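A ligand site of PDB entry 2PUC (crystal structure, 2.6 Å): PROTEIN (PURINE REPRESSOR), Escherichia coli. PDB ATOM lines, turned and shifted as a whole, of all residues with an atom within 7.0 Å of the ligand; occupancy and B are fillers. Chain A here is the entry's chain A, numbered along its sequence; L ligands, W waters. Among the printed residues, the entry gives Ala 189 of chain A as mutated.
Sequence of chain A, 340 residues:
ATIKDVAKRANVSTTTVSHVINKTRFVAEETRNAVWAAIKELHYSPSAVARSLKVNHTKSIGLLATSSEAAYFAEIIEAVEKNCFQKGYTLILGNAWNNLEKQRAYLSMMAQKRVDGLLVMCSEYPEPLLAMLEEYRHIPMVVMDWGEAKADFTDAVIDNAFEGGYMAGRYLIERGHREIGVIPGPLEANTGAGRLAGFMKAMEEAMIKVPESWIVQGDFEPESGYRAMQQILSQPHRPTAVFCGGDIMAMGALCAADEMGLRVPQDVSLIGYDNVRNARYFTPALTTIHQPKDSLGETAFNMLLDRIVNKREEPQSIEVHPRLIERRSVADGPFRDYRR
Water W4 lies within hydrogen-bond range of N2 of the ligand (2.8 Å) and OG1 of Thr 191 (3.0 Å). Water W3 lies within hydrogen-bond range of the backbone carbonyl oxygen (O) of Phe 220 (2.9 Å), a nitrogen (N4) of the ligand (3.2 Å) and the side-chain carboxylate (OE1) of Glu 221 (3.3 Å).
The side-chain hydroxyl of Thr 191 lies within hydrogen-bond range of a nitrogen (N2) of the ligand (2.7 Å). A nitrogen (N1) of the ligand is in hydrogen-bond range of the side-chain carboxylate (OD2) of Asp 274, 2.8 Å away. The side-chain hydroxyl (OG) of Ser 123 sits at hydrogen-bond distance from an oxygen (O1) of the ligand.
Residues that only touch the ligand: Ala 70 (3.4 Å), Tyr 72 (3.4 Å), Phe 73 (3.4 Å), Arg 195 (3.3 Å) and Phe 220 (3.1 Å).
NE of Arg 195 lies close to O of Thr 191, 3.3 Å away. The side-chain carboxylate (OD1) of Asp 274 lies within salt-bridge range of the guanidinium group (NH2) of Arg 195, at 2.6 Å. The backbone carbonyl oxygen (O) of Asp 274 is in hydrogen-bond range of the backbone NH (N) of Gln 291, at 3.2 Å. N of Ser 123 lies within hydrogen-bond range of OD2 of Asp 145, at 3.1 Å. NH1 of Arg 195 lies within hydrogen-bond range of O of Gly 245 (2.8 Å). The side-chain hydroxyl (OH) of Tyr 72 sits at hydrogen-bond distance from the side-chain amide oxygen (OE1) of Gln 291 (3.0 Å).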
ATOM      1  N   THR A  66     -20.240  -8.910  -0.098  1.00  0.00           N
ATOM      2  CA  THR A  66     -21.476  -9.219  -0.772  1.00  0.00           C
ATOM      3  C   THR A  66     -21.241 -10.488  -1.555  1.00  0.00           C
ATOM      4  O   THR A  66     -21.967 -11.473  -1.429  1.00  0.00           O
ATOM      5  CB  THR A  66     -21.803  -8.118  -1.768  1.00  0.00           C
ATOM      6  OG1 THR A  66     -22.581  -7.093  -1.129  1.00  0.00           O
ATOM      7  CG2 THR A  66     -22.583  -8.691  -2.918  1.00  0.00           C
ATOM      8  N   SER A  67     -20.197 -10.450  -2.368  1.00  0.00           N
ATOM      9  CA  SER A  67     -19.845 -11.586  -3.174  1.00  0.00           C
ATOM     10  C   SER A  67     -18.330 -11.506  -3.386  1.00  0.00           C
ATOM     11  O   SER A  67     -17.751 -10.454  -3.307  1.00  0.00           O
ATOM     12  CB  SER A  67     -20.644 -11.562  -4.495  1.00  0.00           C
ATOM     13  OG  SER A  67     -19.816 -11.769  -5.636  1.00  0.00           O
ATOM     14  N   ALA A  70     -17.028 -11.751  -8.274  1.00  0.00           N
ATOM     15  CA  ALA A  70     -16.946 -10.531  -9.090  1.00  0.00           C
ATOM     16  C   ALA A  70     -15.596  -9.838  -9.085  1.00  0.00           C
ATOM     17  O   ALA A  70     -15.086  -9.458  -8.006  1.00  0.00           O
ATOM     18  CB  ALA A  70     -17.997  -9.534  -8.603  1.00  0.00           C
ATOM     19  N   ALA A  71     -15.039  -9.701 -10.297  1.00  0.00           N
ATOM     20  CA  ALA A  71     -13.716  -9.050 -10.523  1.00  0.00           C
ATOM     21  C   ALA A  71     -13.504  -7.908  -9.548  1.00  0.00           C
ATOM     22  O   ALA A  71     -12.593  -7.934  -8.723  1.00  0.00           O
ATOM     23  CB  ALA A  71     -13.609  -8.536 -11.942  1.00  0.00           C
ATOM     24  N   TYR A  72     -14.414  -6.941  -9.635  1.00  0.00           N
ATOM     25  CA  TYR A  72     -14.373  -5.771  -8.807  1.00  0.00           C
ATOM     26  C   TYR A  72     -14.090  -6.153  -7.367  1.00  0.00           C
ATOM     27  O   TYR A  72     -12.984  -5.996  -6.887  1.00  0.00           O
ATOM     28  CB  TYR A  72     -15.688  -5.066  -8.918  1.00  0.00           C
ATOM     29  CG  TYR A  72     -15.713  -3.813  -8.141  1.00  0.00           C
ATOM     30  CD1 TYR A  72     -15.054  -2.703  -8.606  1.00  0.00           C
ATOM     31  CD2 TYR A  72     -16.405  -3.727  -6.960  1.00  0.00           C
ATOM     32  CE1 TYR A  72     -15.070  -1.516  -7.893  1.00  0.00           C
ATOM     33  CE2 TYR A  72     -16.463  -2.548  -6.267  1.00  0.00           C
ATOM     34  CZ  TYR A  72     -15.764  -1.448  -6.736  1.00  0.00           C
ATOM     35  OH  TYR A  72     -15.748  -0.274  -6.068  1.00  0.00           O
ATOM     36  N   PHE A  73     -15.042  -6.801  -6.736  1.00  0.00           N
ATOM     37  CA  PHE A  73     -14.826  -7.240  -5.364  1.00  0.00           C
ATOM     38  C   PHE A  73     -13.597  -8.054  -5.125  1.00  0.00           C
ATOM     39  O   PHE A  73     -12.922  -7.934  -4.125  1.00  0.00           O
ATOM     40  CB  PHE A  73     -15.982  -8.118  -4.977  1.00  0.00           C
ATOM     41  CG  PHE A  73     -17.243  -7.365  -4.920  1.00  0.00           C
ATOM     42  CD1 PHE A  73     -17.270  -6.142  -4.332  1.00  0.00           C
ATOM     43  CD2 PHE A  73     -18.378  -7.851  -5.511  1.00  0.00           C
ATOM     44  CE1 PHE A  73     -18.419  -5.419  -4.277  1.00  0.00           C
ATOM     45  CE2 PHE A  73     -19.547  -7.136  -5.477  1.00  0.00           C
ATOM     46  CZ  PHE A  73     -19.568  -5.908  -4.868  1.00  0.00           C
ATOM     47  N   SER A 123     -22.777  -3.290  -0.485  1.00  0.00           N
ATOM     48  CA  SER A 123     -23.458  -2.752  -1.646  1.00  0.00           C
ATOM     49  C   SER A 123     -24.707  -1.979  -1.382  1.00  0.00           C
ATOM     50  O   SER A 123     -24.704  -0.791  -1.598  1.00  0.00           O
ATOM     51  CB  SER A 123     -23.702  -3.833  -2.670  1.00  0.00           C
ATOM     52  OG  SER A 123     -22.523  -4.022  -3.432  1.00  0.00           O
ATOM     53  N   ASP A 145     -17.962   1.209   1.127  1.00  0.00           N
ATOM     54  CA  ASP A 145     -18.652   1.484  -0.113  1.00  0.00           C
ATOM     55  C   ASP A 145     -19.789   2.478  -0.120  1.00  0.00           C
ATOM     56  O   ASP A 145     -20.636   2.403  -0.989  1.00  0.00           O
ATOM     57  CB  ASP A 145     -19.056   0.167  -0.814  1.00  0.00           C
ATOM     58  CG  ASP A 145     -19.980  -0.731   0.054  1.00  0.00           C
ATOM     59  OD1 ASP A 145     -20.659  -0.194   0.982  1.00  0.00           O
ATOM     60  OD2 ASP A 145     -20.029  -1.961  -0.204  1.00  0.00           O
ATOM     61  N   ASP A 159     -15.467   6.983  -2.441  1.00  0.00           N
ATOM     62  CA  ASP A 159     -14.892   6.835  -3.769  1.00  0.00           C
ATOM     63  C   ASP A 159     -15.177   7.916  -4.792  1.00  0.00           C
ATOM     64  O   ASP A 159     -14.725   7.797  -5.913  1.00  0.00           O
ATOM     65  CB  ASP A 159     -15.314   5.483  -4.322  1.00  0.00           C
ATOM     66  CG  ASP A 159     -16.802   5.442  -4.634  1.00  0.00           C
ATOM     67  OD1 ASP A 159     -17.499   6.452  -4.360  1.00  0.00           O
ATOM     68  OD2 ASP A 159     -17.255   4.422  -5.174  1.00  0.00           O
ATOM     69  N   PRO A 186     -27.197  -1.018 -10.322  1.00  0.00           N
ATOM     70  CA  PRO A 186     -28.323  -0.910  -9.385  1.00  0.00           C
ATOM     71  C   PRO A 186     -28.366   0.406  -8.647  1.00  0.00           C
ATOM     72  O   PRO A 186     -27.400   0.816  -7.988  1.00  0.00           O
ATOM     73  CB  PRO A 186     -28.087  -2.027  -8.397  1.00  0.00           C
ATOM     74  CG  PRO A 186     -27.043  -2.923  -8.987  1.00  0.00           C
ATOM     75  CD  PRO A 186     -26.472  -2.299 -10.221  1.00  0.00           C
ATOM     76  N   ALA A 189     -27.430   0.940  -5.057  1.00  0.00           N
ATOM     77  CA  ALA A 189     -26.020   0.947  -4.686  1.00  0.00           C
ATOM     78  C   ALA A 189     -25.390   2.327  -5.047  1.00  0.00           C
ATOM     79  O   ALA A 189     -25.911   3.074  -5.884  1.00  0.00           O
ATOM     80  CB  ALA A 189     -25.288  -0.232  -5.361  1.00  0.00           C
ATOM     81  N   ASN A 190     -24.298   2.651  -4.382  1.00  0.00           N
ATOM     82  CA  ASN A 190     -23.600   3.900  -4.599  1.00  0.00           C
ATOM     83  C   ASN A 190     -22.976   3.918  -5.981  1.00  0.00           C
ATOM     84  O   ASN A 190     -23.309   4.778  -6.828  1.00  0.00           O
ATOM     85  CB  ASN A 190     -22.501   4.079  -3.544  1.00  0.00           C
ATOM     86  CG  ASN A 190     -21.551   5.231  -3.867  1.00  0.00           C
ATOM     87  OD1 ASN A 190     -22.003   6.392  -4.079  1.00  0.00           O
ATOM     88  ND2 ASN A 190     -20.232   4.937  -3.862  1.00  0.00           N
ATOM     89  N   THR A 191     -22.079   2.959  -6.197  1.00  0.00           N
ATOM     90  CA  THR A 191     -21.386   2.838  -7.465  1.00  0.00           C
ATOM     91  C   THR A 191     -22.385   2.719  -8.608  1.00  0.00           C
ATOM     92  O   THR A 191     -21.967   2.802  -9.770  1.00  0.00           O
ATOM     93  CB  THR A 191     -20.480   1.614  -7.507  1.00  0.00           C
ATOM     94  OG1 THR A 191     -21.300   0.494  -7.279  1.00  0.00           O
ATOM     95  CG2 THR A 191     -19.335   1.626  -6.455  1.00  0.00           C
ATOM     96  N   GLY A 192     -23.687   2.532  -8.286  1.00  0.00           N
ATOM     97  CA  GLY A 192     -24.729   2.466  -9.303  1.00  0.00           C
ATOM     98  C   GLY A 192     -25.333   3.864  -9.492  1.00  0.00           C
ATOM     99  O   GLY A 192     -25.153   4.532 -10.510  1.00  0.00           O
ATOM    100  N   ARG A 195     -22.819   6.935  -9.930  1.00  0.00           N
ATOM    101  CA  ARG A 195     -22.065   7.157 -11.149  1.00  0.00           C
ATOM    102  C   ARG A 195     -23.026   7.680 -12.204  1.00  0.00           C
ATOM    103  O   ARG A 195     -22.666   8.442 -13.082  1.00  0.00           O
ATOM    104  CB  ARG A 195     -21.331   5.872 -11.599  1.00  0.00           C
ATOM    105  CG  ARG A 195     -20.284   5.249 -10.599  1.00  0.00           C
ATOM    106  CD  ARG A 195     -19.701   3.872 -11.088  1.00  0.00           C
ATOM    107  NE  ARG A 195     -18.734   3.325 -10.130  1.00  0.00           N
ATOM    108  CZ  ARG A 195     -18.236   2.087 -10.209  1.00  0.00           C
ATOM    109  NH1 ARG A 195     -18.617   1.293 -11.211  1.00  0.00           N
ATOM    110  NH2 ARG A 195     -17.371   1.642  -9.297  1.00  0.00           N
ATOM    111  N   ASP A 219     -26.886  -5.006 -13.598  1.00  0.00           N
ATOM    112  CA  ASP A 219     -26.663  -5.414 -12.220  1.00  0.00           C
ATOM    113  C   ASP A 219     -25.183  -5.697 -11.979  1.00  0.00           C
ATOM    114  O   ASP A 219     -24.854  -6.407 -11.032  1.00  0.00           O
ATOM    115  CB  ASP A 219     -27.492  -6.659 -11.903  1.00  0.00           C
ATOM    116  CG  ASP A 219     -27.243  -7.802 -12.887  1.00  0.00           C
ATOM    117  OD1 ASP A 219     -26.184  -7.865 -13.546  1.00  0.00           O
ATOM    118  OD2 ASP A 219     -28.109  -8.686 -12.958  1.00  0.00           O
ATOM    119  N   PHE A 220     -24.306  -5.159 -12.830  1.00  0.00           N
ATOM    120  CA  PHE A 220     -22.837  -5.407 -12.775  1.00  0.00           C
ATOM    121  C   PHE A 220     -22.473  -6.791 -13.373  1.00  0.00           C
ATOM    122  O   PHE A 220     -21.314  -7.122 -13.508  1.00  0.00           O
ATOM    123  CB  PHE A 220     -22.298  -5.307 -11.342  1.00  0.00           C
ATOM    124  CG  PHE A 220     -22.335  -3.917 -10.814  1.00  0.00           C
ATOM    125  CD1 PHE A 220     -21.757  -2.898 -11.526  1.00  0.00           C
ATOM    126  CD2 PHE A 220     -23.017  -3.626  -9.636  1.00  0.00           C
ATOM    127  CE1 PHE A 220     -21.789  -1.606 -11.057  1.00  0.00           C
ATOM    128  CE2 PHE A 220     -23.072  -2.333  -9.166  1.00  0.00           C
ATOM    129  CZ  PHE A 220     -22.453  -1.327  -9.872  1.00  0.00           C
ATOM    130  N   GLU A 221     -23.470  -7.585 -13.694  1.00  0.00           N
ATOM    131  CA  GLU A 221     -23.185  -8.893 -14.263  1.00  0.00           C
ATOM    132  C   GLU A 221     -23.265  -8.852 -15.770  1.00  0.00           C
ATOM    133  O   GLU A 221     -24.175  -8.309 -16.385  1.00  0.00           O
ATOM    134  CB  GLU A 221     -24.140  -9.907 -13.670  1.00  0.00           C
ATOM    135  CG  GLU A 221     -23.871 -10.159 -12.195  1.00  0.00           C
ATOM    136  CD  GLU A 221     -22.919 -11.299 -11.969  1.00  0.00           C
ATOM    137  OE1 GLU A 221     -21.695 -11.091 -12.129  1.00  0.00           O
ATOM    138  OE2 GLU A 221     -23.395 -12.416 -11.629  1.00  0.00           O
ATOM    139  N   GLY A 245     -21.920   1.514 -16.590  1.00  0.00           N
ATOM    140  CA  GLY A 245     -21.465   1.622 -15.202  1.00  0.00           C
ATOM    141  C   GLY A 245     -20.555   0.602 -14.522  1.00  0.00           C
ATOM    142  O   GLY A 245     -20.430   0.625 -13.303  1.00  0.00           O
ATOM    143  N   GLY A 246     -19.940  -0.310 -15.272  1.00  0.00           N
ATOM    144  CA  GLY A 246     -19.102  -1.370 -14.678  1.00  0.00           C
ATOM    145  C   GLY A 246     -18.391  -2.141 -15.805  1.00  0.00           C
ATOM    146  O   GLY A 246     -19.007  -2.503 -16.823  1.00  0.00           O
ATOM    147  N   ASP A 247     -17.104  -2.391 -15.657  1.00  0.00           N
ATOM    148  CA  ASP A 247     -16.387  -3.074 -16.696  1.00  0.00           C
ATOM    149  C   ASP A 247     -16.944  -4.461 -17.115  1.00  0.00           C
ATOM    150  O   ASP A 247     -17.042  -4.795 -18.314  1.00  0.00           O
ATOM    151  CB  ASP A 247     -14.925  -3.179 -16.329  1.00  0.00           C
ATOM    152  CG  ASP A 247     -14.176  -1.844 -16.461  1.00  0.00           C
ATOM    153  OD1 ASP A 247     -14.784  -0.843 -16.868  1.00  0.00           O
ATOM    154  OD2 ASP A 247     -12.974  -1.804 -16.122  1.00  0.00           O
ATOM    155  N   ILE A 248     -17.299  -5.268 -16.123  1.00  0.00           N
ATOM    156  CA  ILE A 248     -17.804  -6.596 -16.433  1.00  0.00           C
ATOM    157  C   ILE A 248     -19.102  -6.522 -17.234  1.00  0.00           C
ATOM    158  O   ILE A 248     -19.305  -7.265 -18.177  1.00  0.00           O
ATOM    159  CB  ILE A 248     -17.915  -7.483 -15.236  1.00  0.00           C
ATOM    160  CG1 ILE A 248     -16.603  -7.529 -14.440  1.00  0.00           C
ATOM    161  CG2 ILE A 248     -18.394  -8.883 -15.632  1.00  0.00           C
ATOM    162  CD1 ILE A 248     -15.446  -8.170 -15.143  1.00  0.00           C
ATOM    163  N   TYR A 273     -16.156   1.453 -16.545  1.00  0.00           N
ATOM    164  CA  TYR A 273     -15.941   1.983 -15.235  1.00  0.00           C
ATOM    165  C   TYR A 273     -15.525   0.875 -14.307  1.00  0.00           C
ATOM    166  O   TYR A 273     -16.297  -0.103 -14.126  1.00  0.00           O
ATOM    167  CB  TYR A 273     -17.229   2.534 -14.674  1.00  0.00           C
ATOM    168  CG  TYR A 273     -16.957   3.519 -13.579  1.00  0.00           C
ATOM    169  CD1 TYR A 273     -16.103   3.200 -12.530  1.00  0.00           C
ATOM    170  CD2 TYR A 273     -17.488   4.817 -13.618  1.00  0.00           C
ATOM    171  CE1 TYR A 273     -15.824   4.125 -11.538  1.00  0.00           C
ATOM    172  CE2 TYR A 273     -17.224   5.740 -12.635  1.00  0.00           C
ATOM    173  CZ  TYR A 273     -16.390   5.389 -11.602  1.00  0.00           C
ATOM    174  OH  TYR A 273     -16.099   6.323 -10.639  1.00  0.00           O
ATOM    175  N   ASP A 274     -14.346   1.065 -13.713  1.00  0.00           N
ATOM    176  CA  ASP A 274     -13.684   0.241 -12.676  1.00  0.00           C
ATOM    177  C   ASP A 274     -12.209  -0.017 -12.970  1.00  0.00           C
ATOM    178  O   ASP A 274     -11.346  -0.083 -12.088  1.00  0.00           O
ATOM    179  CB  ASP A 274     -14.400  -1.097 -12.413  1.00  0.00           C
ATOM    180  CG  ASP A 274     -15.730  -0.972 -11.573  1.00  0.00           C
ATOM    181  OD1 ASP A 274     -16.089   0.100 -11.013  1.00  0.00           O
ATOM    182  OD2 ASP A 274     -16.436  -2.006 -11.508  1.00  0.00           O
ATOM    183  N   VAL A 276     -10.986  -2.799 -14.139  1.00  0.00           N
ATOM    184  CA  VAL A 276     -10.714  -4.091 -13.522  1.00  0.00           C
ATOM    185  C   VAL A 276      -9.420  -4.666 -14.109  1.00  0.00           C
ATOM    186  O   VAL A 276      -9.138  -4.489 -15.296  1.00  0.00           O
ATOM    187  CB  VAL A 276     -11.914  -5.024 -13.836  1.00  0.00           C
ATOM    188  CG1 VAL A 276     -11.443  -6.417 -14.249  1.00  0.00           C
ATOM    189  CG2 VAL A 276     -12.877  -5.073 -12.643  1.00  0.00           C
ATOM    190  N   GLN A 291     -10.851   2.856 -10.793  1.00  0.00           N
ATOM    191  CA  GLN A 291     -11.174   2.973  -9.385  1.00  0.00           C
ATOM    192  C   GLN A 291      -9.998   2.398  -8.670  1.00  0.00           C
ATOM    193  O   GLN A 291      -9.533   1.299  -8.997  1.00  0.00           O
ATOM    194  CB  GLN A 291     -12.375   2.123  -9.011  1.00  0.00           C
ATOM    195  CG  GLN A 291     -12.656   2.115  -7.486  1.00  0.00           C
ATOM    196  CD  GLN A 291     -13.848   3.007  -7.070  1.00  0.00           C
ATOM    197  OE1 GLN A 291     -14.834   2.562  -6.491  1.00  0.00           O
ATOM    198  NE2 GLN A 291     -13.725   4.293  -7.316  1.00  0.00           N
HETATM  199  N1  LIG L   1     -18.440  -2.237  -9.561  1.00  0.00           N
HETATM  200  C1  LIG L   1     -18.897  -1.228  -8.751  1.00  0.00           C
HETATM  201  N2  LIG L   1     -19.788  -1.631  -7.884  1.00  0.00           N
HETATM  202  C2  LIG L   1     -19.936  -2.979  -8.138  1.00  0.00           C
HETATM  203  C3  LIG L   1     -20.765  -3.943  -7.513  1.00  0.00           C
HETATM  204  O1  LIG L   1     -21.571  -3.800  -6.579  1.00  0.00           O
HETATM  205  N3  LIG L   1     -20.599  -5.195  -8.074  1.00  0.00           N
HETATM  206  C4  LIG L   1     -19.750  -5.499  -9.112  1.00  0.00           C
HETATM  207  N4  LIG L   1     -19.749  -6.781  -9.526  1.00  0.00           N
HETATM  208  N5  LIG L   1     -18.973  -4.614  -9.708  1.00  0.00           N
HETATM  209  C5  LIG L   1     -19.105  -3.380  -9.163  1.00  0.00           C
HETATM  210  O   HOH W   1     -16.960  -6.887 -11.046  1.00  0.00           O
HETATM  211  O   HOH W   2     -22.871  -6.676  -6.945  1.00  0.00           O
HETATM  212  O   HOH W   3     -19.387  -8.723 -12.074  1.00  0.00           O
HETATM  213  O   HOH W   4     -20.287  -1.383  -5.125  1.00  0.00           O
